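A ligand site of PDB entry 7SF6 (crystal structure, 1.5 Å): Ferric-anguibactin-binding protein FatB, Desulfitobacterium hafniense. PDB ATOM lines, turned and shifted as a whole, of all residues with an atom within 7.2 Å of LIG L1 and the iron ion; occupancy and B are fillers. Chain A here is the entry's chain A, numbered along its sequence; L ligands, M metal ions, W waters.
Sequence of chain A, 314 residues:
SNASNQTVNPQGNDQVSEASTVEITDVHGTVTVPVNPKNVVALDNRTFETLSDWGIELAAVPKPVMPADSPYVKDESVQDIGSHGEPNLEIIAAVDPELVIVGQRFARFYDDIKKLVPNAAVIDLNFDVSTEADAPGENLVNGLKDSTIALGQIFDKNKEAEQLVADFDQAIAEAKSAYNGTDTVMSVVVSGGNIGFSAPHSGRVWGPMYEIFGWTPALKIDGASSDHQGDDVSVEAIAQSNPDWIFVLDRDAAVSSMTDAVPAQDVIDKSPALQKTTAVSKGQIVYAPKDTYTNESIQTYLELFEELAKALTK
Residues that only touch LIG L1: Gln 104. Of the 20 residues printed, 6 come within 4 Å of LIG L1.
NH2 of Arg 108 is in hydrogen-bond range of O of His 84, at 2.9 Å. NE of Arg 204 lies within salt-bridge range of OE2 of Glu 296, 2.9 Å away. The backbone carbonyl oxygen of Tyr 293 lies close to the guanidinium group of Arg 204, 3.4 Å away. The side-chain amide oxygen (OD1) of Asn 45 sits close to the guanidinium group (NH1) of Arg 105, at 3.2 Å. NH1 of Arg 105 is in hydrogen-bond range of OE1 of Gln 104 (3.3 Å). The guanidinium group (NH2) of Arg 105 is in hydrogen-bond range of the backbone carbonyl oxygen (O) of Tyr 293 (2.8 Å). The side-chain amide nitrogen of Gln 104 lies within hydrogen-bond range of the side-chain carboxylate of Glu 296, 2.9 Å away. The guanidinium group (NE) of Arg 251 lies close to the side-chain hydroxyl (OH) of Tyr 293 (2.7 Å).
The iron ion is bound by OH of Tyr 293 (2.0 Å), O1 of LG2 L2 (2.0 Å), O1 of LIG L1 (2.1 Å), O2 of LIG L1 (2.1 Å), O2 of LG2 L2 (2.1 Å) and ND1 of His 228 (2.3 Å).
O2 of LIG L1 sits close to NE2 of His 84 (3.0 Å). The guanidinium group (NE) of Arg 105 sits close to an oxygen (O1) of LG2 L2, 2.8 Å away. The guanidinium group of Arg 251 lies within salt-bridge range of an oxygen (O6) of LG2 L2 (2.8 Å). NH2 of Arg 105 lies close to O1 of LIG L1 (3.5 Å). O1 of LIG L1 sits close to NH1 of Arg 204 (2.8 Å).
Water W3 lies within hydrogen-bond range of an oxygen (O3) of LIG L1 (2.5 Å), the backbone carbonyl oxygen of Arg 105 (2.7 Å) and the guanidinium group of Arg 108 (2.9 Å).
Two residues have an atom within 4 Å of the iron ion: His 228 and Tyr 293.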
ATOM      1  N   ASN A  45       9.052  27.032 -30.285  1.00  0.00           N
ATOM      2  CA  ASN A  45       9.102  25.577 -30.226  1.00  0.00           C
ATOM      3  C   ASN A  45       7.887  24.948 -30.895  1.00  0.00           C
ATOM      4  O   ASN A  45       7.988  23.777 -31.307  1.00  0.00           O
ATOM      5  CB  ASN A  45       9.124  25.090 -28.763  1.00  0.00           C
ATOM      6  CG  ASN A  45      10.518  25.204 -28.158  1.00  0.00           C
ATOM      7  OD1 ASN A  45      10.892  26.251 -27.597  1.00  0.00           O
ATOM      8  ND2 ASN A  45      11.288  24.131 -28.264  1.00  0.00           N
ATOM      9  N   HIS A  84      16.984  29.710 -23.571  1.00  0.00           N
ATOM     10  CA  HIS A  84      16.011  30.732 -23.235  1.00  0.00           C
ATOM     11  C   HIS A  84      16.350  31.413 -21.922  1.00  0.00           C
ATOM     12  O   HIS A  84      15.902  32.532 -21.714  1.00  0.00           O
ATOM     13  CB  HIS A  84      14.564  30.212 -23.252  1.00  0.00           C
ATOM     14  CG  HIS A  84      14.278  29.101 -22.299  1.00  0.00           C
ATOM     15  ND1 HIS A  84      15.120  28.025 -22.104  1.00  0.00           N
ATOM     16  CD2 HIS A  84      13.196  28.872 -21.512  1.00  0.00           C
ATOM     17  CE1 HIS A  84      14.558  27.178 -21.268  1.00  0.00           C
ATOM     18  NE2 HIS A  84      13.389  27.670 -20.873  1.00  0.00           N
ATOM     19  N   GLY A  85      17.132  30.765 -21.058  1.00  0.00           N
ATOM     20  CA  GLY A  85      17.541  31.408 -19.830  1.00  0.00           C
ATOM     21  C   GLY A  85      18.648  32.407 -20.021  1.00  0.00           C
ATOM     22  O   GLY A  85      18.761  33.388 -19.265  1.00  0.00           O
ATOM     23  N   GLY A 103       7.982  32.740 -30.147  1.00  0.00           N
ATOM     24  CA  GLY A 103       6.952  31.914 -29.539  1.00  0.00           C
ATOM     25  C   GLY A 103       7.415  31.501 -28.154  1.00  0.00           C
ATOM     26  O   GLY A 103       8.460  31.942 -27.670  1.00  0.00           O
ATOM     27  N   GLN A 104       6.595  30.652 -27.535  1.00  0.00           N
ATOM     28  CA  GLN A 104       6.662  30.064 -26.189  1.00  0.00           C
ATOM     29  C   GLN A 104       7.818  30.521 -25.291  1.00  0.00           C
ATOM     30  O   GLN A 104       7.676  31.446 -24.453  1.00  0.00           O
ATOM     31  CB  GLN A 104       6.639  28.529 -26.346  1.00  0.00           C
ATOM     32  CG  GLN A 104       6.454  27.793 -25.067  1.00  0.00           C
ATOM     33  CD  GLN A 104       6.367  26.295 -25.267  1.00  0.00           C
ATOM     34  OE1 GLN A 104       6.956  25.751 -26.234  1.00  0.00           O
ATOM     35  NE2 GLN A 104       5.684  25.596 -24.373  1.00  0.00           N
ATOM     36  N   ARG A 105       9.007  29.926 -25.464  1.00  0.00           N
ATOM     37  CA  ARG A 105      10.103  30.186 -24.512  1.00  0.00           C
ATOM     38  C   ARG A 105      10.767  31.536 -24.708  1.00  0.00           C
ATOM     39  O   ARG A 105      11.581  31.938 -23.839  1.00  0.00           O
ATOM     40  CB  ARG A 105      11.131  29.070 -24.609  1.00  0.00           C
ATOM     41  CG  ARG A 105      10.597  27.716 -24.050  1.00  0.00           C
ATOM     42  CD  ARG A 105      11.637  26.639 -24.223  1.00  0.00           C
ATOM     43  NE  ARG A 105      11.258  25.436 -23.486  1.00  0.00           N
ATOM     44  CZ  ARG A 105      10.441  24.464 -23.890  1.00  0.00           C
ATOM     45  NH1 ARG A 105       9.818  24.511 -25.088  1.00  0.00           N
ATOM     46  NH2 ARG A 105      10.328  23.357 -23.132  1.00  0.00           N
ATOM     47  N   PHE A 106      10.489  32.213 -25.819  1.00  0.00           N
ATOM     48  CA  PHE A 106      11.074  33.517 -26.086  1.00  0.00           C
ATOM     49  C   PHE A 106      10.053  34.645 -26.029  1.00  0.00           C
ATOM     50  O   PHE A 106      10.386  35.797 -26.322  1.00  0.00           O
ATOM     51  CB  PHE A 106      11.860  33.520 -27.410  1.00  0.00           C
ATOM     52  CG  PHE A 106      13.191  32.827 -27.298  1.00  0.00           C
ATOM     53  CD1 PHE A 106      13.277  31.424 -27.264  1.00  0.00           C
ATOM     54  CD2 PHE A 106      14.338  33.587 -27.086  1.00  0.00           C
ATOM     55  CE1 PHE A 106      14.516  30.815 -27.032  1.00  0.00           C
ATOM     56  CE2 PHE A 106      15.589  32.975 -26.888  1.00  0.00           C
ATOM     57  CZ  PHE A 106      15.657  31.584 -26.858  1.00  0.00           C
ATOM     58  N   ALA A 107       8.846  34.340 -25.585  1.00  0.00           N
ATOM     59  CA  ALA A 107       7.793  35.355 -25.518  1.00  0.00           C
ATOM     60  C   ALA A 107       8.208  36.558 -24.685  1.00  0.00           C
ATOM     61  O   ALA A 107       7.897  37.693 -25.029  1.00  0.00           O
ATOM     62  CB  ALA A 107       6.502  34.707 -24.999  1.00  0.00           C
ATOM     63  N   ARG A 108       8.930  36.336 -23.600  1.00  0.00           N
ATOM     64  CA  ARG A 108       9.280  37.458 -22.734  1.00  0.00           C
ATOM     65  C   ARG A 108      10.296  38.395 -23.375  1.00  0.00           C
ATOM     66  O   ARG A 108      10.518  39.490 -22.848  1.00  0.00           O
ATOM     67  CB  ARG A 108       9.821  36.925 -21.402  1.00  0.00           C
ATOM     68  CG  ARG A 108      11.147  36.251 -21.493  1.00  0.00           C
ATOM     69  CD  ARG A 108      11.480  35.713 -20.148  1.00  0.00           C
ATOM     70  NE  ARG A 108      12.673  34.883 -20.224  1.00  0.00           N
ATOM     71  CZ  ARG A 108      13.836  35.239 -19.708  1.00  0.00           C
ATOM     72  NH1 ARG A 108      14.012  36.448 -19.166  1.00  0.00           N
ATOM     73  NH2 ARG A 108      14.845  34.355 -19.713  1.00  0.00           N
ATOM     74  N   PHE A 109      10.890  37.989 -24.486  1.00  0.00           N
ATOM     75  CA  PHE A 109      11.851  38.813 -25.187  1.00  0.00           C
ATOM     76  C   PHE A 109      11.268  39.595 -26.345  1.00  0.00           C
ATOM     77  O   PHE A 109      12.029  40.209 -27.096  1.00  0.00           O
ATOM     78  CB  PHE A 109      13.033  37.959 -25.664  1.00  0.00           C
ATOM     79  CG  PHE A 109      13.796  37.338 -24.538  1.00  0.00           C
ATOM     80  CD1 PHE A 109      14.528  38.123 -23.654  1.00  0.00           C
ATOM     81  CD2 PHE A 109      13.793  35.952 -24.359  1.00  0.00           C
ATOM     82  CE1 PHE A 109      15.267  37.514 -22.584  1.00  0.00           C
ATOM     83  CE2 PHE A 109      14.486  35.352 -23.300  1.00  0.00           C
ATOM     84  CZ  PHE A 109      15.236  36.139 -22.439  1.00  0.00           C
ATOM     85  N   ASN A 126       3.194  33.192 -29.551  1.00  0.00           N
ATOM     86  CA  ASN A 126       2.878  32.648 -28.222  1.00  0.00           C
ATOM     87  C   ASN A 126       1.421  32.965 -27.874  1.00  0.00           C
ATOM     88  O   ASN A 126       0.986  34.111 -27.943  1.00  0.00           O
ATOM     89  CB  ASN A 126       3.811  33.264 -27.184  1.00  0.00           C
ATOM     90  CG  ASN A 126       3.592  32.671 -25.801  1.00  0.00           C
ATOM     91  OD1 ASN A 126       3.702  31.438 -25.614  1.00  0.00           O
ATOM     92  ND2 ASN A 126       3.303  33.533 -24.837  1.00  0.00           N
ATOM     93  N   ARG A 204       1.027  22.218 -17.554  1.00  0.00           N
ATOM     94  CA  ARG A 204       1.863  22.147 -18.769  1.00  0.00           C
ATOM     95  C   ARG A 204       1.470  20.932 -19.620  1.00  0.00           C
ATOM     96  O   ARG A 204       1.353  19.811 -19.105  1.00  0.00           O
ATOM     97  CB  ARG A 204       3.349  22.075 -18.341  1.00  0.00           C
ATOM     98  CG  ARG A 204       4.338  21.956 -19.521  1.00  0.00           C
ATOM     99  CD  ARG A 204       4.151  23.187 -20.500  1.00  0.00           C
ATOM    100  NE  ARG A 204       5.233  23.210 -21.483  1.00  0.00           N
ATOM    101  CZ  ARG A 204       6.466  23.648 -21.209  1.00  0.00           C
ATOM    102  NH1 ARG A 204       6.746  24.201 -20.013  1.00  0.00           N
ATOM    103  NH2 ARG A 204       7.437  23.493 -22.114  1.00  0.00           N
ATOM    104  N   SER A 226       1.104  26.753 -13.903  1.00  0.00           N
ATOM    105  CA  SER A 226       1.565  26.177 -15.159  1.00  0.00           C
ATOM    106  C   SER A 226       2.999  25.671 -15.060  1.00  0.00           C
ATOM    107  O   SER A 226       3.680  25.476 -16.092  1.00  0.00           O
ATOM    108  CB  SER A 226       1.495  27.180 -16.308  1.00  0.00           C
ATOM    109  OG  SER A 226       0.180  27.601 -16.480  1.00  0.00           O
ATOM    110  N   ASP A 227       3.473  25.455 -13.837  1.00  0.00           N
ATOM    111  CA  ASP A 227       4.885  25.102 -13.581  1.00  0.00           C
ATOM    112  C   ASP A 227       5.373  24.073 -14.588  1.00  0.00           C
ATOM    113  O   ASP A 227       4.728  23.044 -14.806  1.00  0.00           O
ATOM    114  CB  ASP A 227       4.956  24.538 -12.156  1.00  0.00           C
ATOM    115  CG  ASP A 227       6.371  24.353 -11.619  1.00  0.00           C
ATOM    116  OD1 ASP A 227       7.317  23.973 -12.345  1.00  0.00           O
ATOM    117  OD2 ASP A 227       6.507  24.524 -10.378  1.00  0.00           O
ATOM    118  N   HIS A 228       6.500  24.374 -15.228  1.00  0.00           N
ATOM    119  CA  HIS A 228       6.998  23.460 -16.240  1.00  0.00           C
ATOM    120  C   HIS A 228       7.394  22.108 -15.703  1.00  0.00           C
ATOM    121  O   HIS A 228       7.529  21.170 -16.502  1.00  0.00           O
ATOM    122  CB  HIS A 228       8.133  24.076 -17.096  1.00  0.00           C
ATOM    123  CG  HIS A 228       9.380  24.430 -16.354  1.00  0.00           C
ATOM    124  ND1 HIS A 228      10.513  24.853 -17.028  1.00  0.00           N
ATOM    125  CD2 HIS A 228       9.662  24.550 -15.025  1.00  0.00           C
ATOM    126  CE1 HIS A 228      11.462  25.149 -16.145  1.00  0.00           C
ATOM    127  NE2 HIS A 228      10.976  24.991 -14.921  1.00  0.00           N
ATOM    128  N   GLN A 229       7.579  21.966 -14.381  1.00  0.00           N
ATOM    129  CA  GLN A 229       7.837  20.660 -13.757  1.00  0.00           C
ATOM    130  C   GLN A 229       6.599  20.079 -13.094  1.00  0.00           C
ATOM    131  O   GLN A 229       6.690  19.046 -12.384  1.00  0.00           O
ATOM    132  CB  GLN A 229       8.995  20.762 -12.760  1.00  0.00           C
ATOM    133  CG  GLN A 229      10.303  21.069 -13.461  1.00  0.00           C
ATOM    134  CD  GLN A 229      11.401  21.253 -12.506  1.00  0.00           C
ATOM    135  OE1 GLN A 229      11.531  22.294 -11.925  1.00  0.00           O
ATOM    136  NE2 GLN A 229      12.174  20.208 -12.281  1.00  0.00           N
ATOM    137  N   ARG A 251       9.444  15.284 -19.115  1.00  0.00           N
ATOM    138  CA  ARG A 251      10.117  16.553 -19.385  1.00  0.00           C
ATOM    139  C   ARG A 251      11.569  16.323 -19.805  1.00  0.00           C
ATOM    140  O   ARG A 251      12.012  16.794 -20.871  1.00  0.00           O
ATOM    141  CB  ARG A 251      10.030  17.447 -18.135  1.00  0.00           C
ATOM    142  CG  ARG A 251      10.894  18.707 -18.221  1.00  0.00           C
ATOM    143  CD  ARG A 251      10.538  19.677 -17.073  1.00  0.00           C
ATOM    144  NE  ARG A 251      11.334  20.911 -17.164  1.00  0.00           N
ATOM    145  CZ  ARG A 251      12.514  21.099 -16.567  1.00  0.00           C
ATOM    146  NH1 ARG A 251      13.010  20.206 -15.683  1.00  0.00           N
ATOM    147  NH2 ARG A 251      13.199  22.224 -16.823  1.00  0.00           N
ATOM    148  N   VAL A 255      14.884  17.261 -23.418  1.00  0.00           N
ATOM    149  CA  VAL A 255      15.852  18.320 -23.248  1.00  0.00           C
ATOM    150  C   VAL A 255      17.254  17.763 -23.521  1.00  0.00           C
ATOM    151  O   VAL A 255      17.734  16.889 -22.797  1.00  0.00           O
ATOM    152  CB  VAL A 255      15.766  18.924 -21.841  1.00  0.00           C
ATOM    153  CG1 VAL A 255      16.887  19.974 -21.751  1.00  0.00           C
ATOM    154  CG2 VAL A 255      14.412  19.601 -21.619  1.00  0.00           C
ATOM    155  N   TYR A 293       7.902  17.903 -24.729  1.00  0.00           N
ATOM    156  CA  TYR A 293       8.201  19.091 -23.921  1.00  0.00           C
ATOM    157  C   TYR A 293       8.942  20.185 -24.695  1.00  0.00           C
ATOM    158  O   TYR A 293       8.767  21.373 -24.392  1.00  0.00           O
ATOM    159  CB  TYR A 293       8.972  18.667 -22.665  1.00  0.00           C
ATOM    160  CG  TYR A 293       9.356  19.805 -21.728  1.00  0.00           C
ATOM    161  CD1 TYR A 293       8.440  20.346 -20.810  1.00  0.00           C
ATOM    162  CD2 TYR A 293      10.684  20.281 -21.690  1.00  0.00           C
ATOM    163  CE1 TYR A 293       8.828  21.341 -19.919  1.00  0.00           C
ATOM    164  CE2 TYR A 293      11.064  21.281 -20.797  1.00  0.00           C
ATOM    165  CZ  TYR A 293      10.138  21.784 -19.908  1.00  0.00           C
ATOM    166  OH  TYR A 293      10.505  22.744 -19.012  1.00  0.00           O
ATOM    167  N   GLU A 296       5.834  21.210 -28.673  1.00  0.00           N
ATOM    168  CA  GLU A 296       4.378  21.209 -28.414  1.00  0.00           C
ATOM    169  C   GLU A 296       3.658  21.742 -29.652  1.00  0.00           C
ATOM    170  O   GLU A 296       3.138  22.857 -29.693  1.00  0.00           O
ATOM    171  CB  GLU A 296       4.049  22.002 -27.179  1.00  0.00           C
ATOM    172  CG  GLU A 296       4.548  21.336 -25.904  1.00  0.00           C
ATOM    173  CD  GLU A 296       4.548  22.316 -24.742  1.00  0.00           C
ATOM    174  OE1 GLU A 296       3.442  22.649 -24.220  1.00  0.00           O
ATOM    175  OE2 GLU A 296       5.645  22.727 -24.305  1.00  0.00           O
HETATM  176  O1  LIG L   1       9.363  25.194 -20.318  1.00  0.00           O
HETATM  177  C1  LIG L   1       9.226  26.524 -20.550  1.00  0.00           C
HETATM  178  C2  LIG L   1       8.184  26.990 -21.363  1.00  0.00           C
HETATM  179  C3  LIG L   1      10.103  27.387 -19.901  1.00  0.00           C
HETATM  180  O2  LIG L   1      11.096  26.817 -19.147  1.00  0.00           O
HETATM  181  C4  LIG L   1       9.934  28.766 -20.062  1.00  0.00           C
HETATM  182  C5  LIG L   1       8.871  29.242 -20.849  1.00  0.00           C
HETATM  183  C6  LIG L   1       8.013  28.364 -21.484  1.00  0.00           C
HETATM  184  C7  LIG L   1      10.754  29.750 -19.300  1.00  0.00           C
HETATM  185  O3  LIG L   1      10.621  30.970 -19.455  1.00  0.00           O
HETATM  186  N1  LIG L   1      11.516  29.249 -18.333  1.00  0.00           N
HETATM  187  C8  LIG L   1      12.212  30.140 -17.427  1.00  0.00           C
HETATM  188  C9  LIG L   1      11.175  30.700 -16.390  1.00  0.00           C
HETATM  189  O4  LIG L   1      10.375  29.735 -15.636  1.00  0.00           O
HETATM  190  C10 LIG L   1      13.125  29.356 -16.576  1.00  0.00           C
HETATM  191  O5  LIG L   1      13.532  29.899 -15.498  1.00  0.00           O
HETATM  192  O6  LIG L   1      13.469  28.211 -16.971  1.00  0.00           O
HETATM  193  O1  LG2 L   2      11.941  24.391 -21.031  1.00  0.00           O
HETATM  194  C1  LG2 L   2      13.262  24.053 -20.965  1.00  0.00           C
HETATM  195  C2  LG2 L   2      13.975  23.644 -22.118  1.00  0.00           C
HETATM  196  C3  LG2 L   2      13.889  24.143 -19.723  1.00  0.00           C
HETATM  197  O2  LG2 L   2      13.097  24.550 -18.693  1.00  0.00           O
HETATM  198  C4  LG2 L   2      15.245  23.871 -19.605  1.00  0.00           C
HETATM  199  C5  LG2 L   2      15.950  23.479 -20.742  1.00  0.00           C
HETATM  200  C6  LG2 L   2      15.352  23.346 -21.999  1.00  0.00           C
HETATM  201  C7  LG2 L   2      16.002  24.052 -18.332  1.00  0.00           C
HETATM  202  O3  LG2 L   2      17.248  23.796 -18.316  1.00  0.00           O
HETATM  203  N1  LG2 L   2      15.365  24.644 -17.303  1.00  0.00           N
HETATM  204  C8  LG2 L   2      16.183  24.940 -16.106  1.00  0.00           C
HETATM  205  C9  LG2 L   2      15.781  26.339 -15.669  1.00  0.00           C
HETATM  206  O4  LG2 L   2      14.395  26.317 -15.344  1.00  0.00           O
HETATM  207  C10 LG2 L   2      16.060  23.939 -14.986  1.00  0.00           C
HETATM  208  O5  LG2 L   2      16.728  24.137 -13.944  1.00  0.00           O
HETATM  209  O6  LG2 L   2      15.283  22.953 -15.129  1.00  0.00           O
HETATM  210 FE    FE M   1      11.029  24.692 -19.224  1.00  0.00          FE
HETATM  211  O   HOH W   1      11.236  28.475 -13.119  1.00  0.00           O
HETATM  212  O   HOH W   2       9.046  27.699 -16.875  1.00  0.00           O
HETATM  213  O   HOH W   3      11.850  32.335 -21.217  1.00  0.00           O
HETATM  214  O   HOH W   4      15.429  29.215 -18.394  1.00  0.00           O
HETATM  215  O   HOH W   5       8.617  32.934 -19.628  1.00  0.00           O
HETATM  216  O   HOH W   6      15.936  29.445 -13.974  1.00  0.00           O
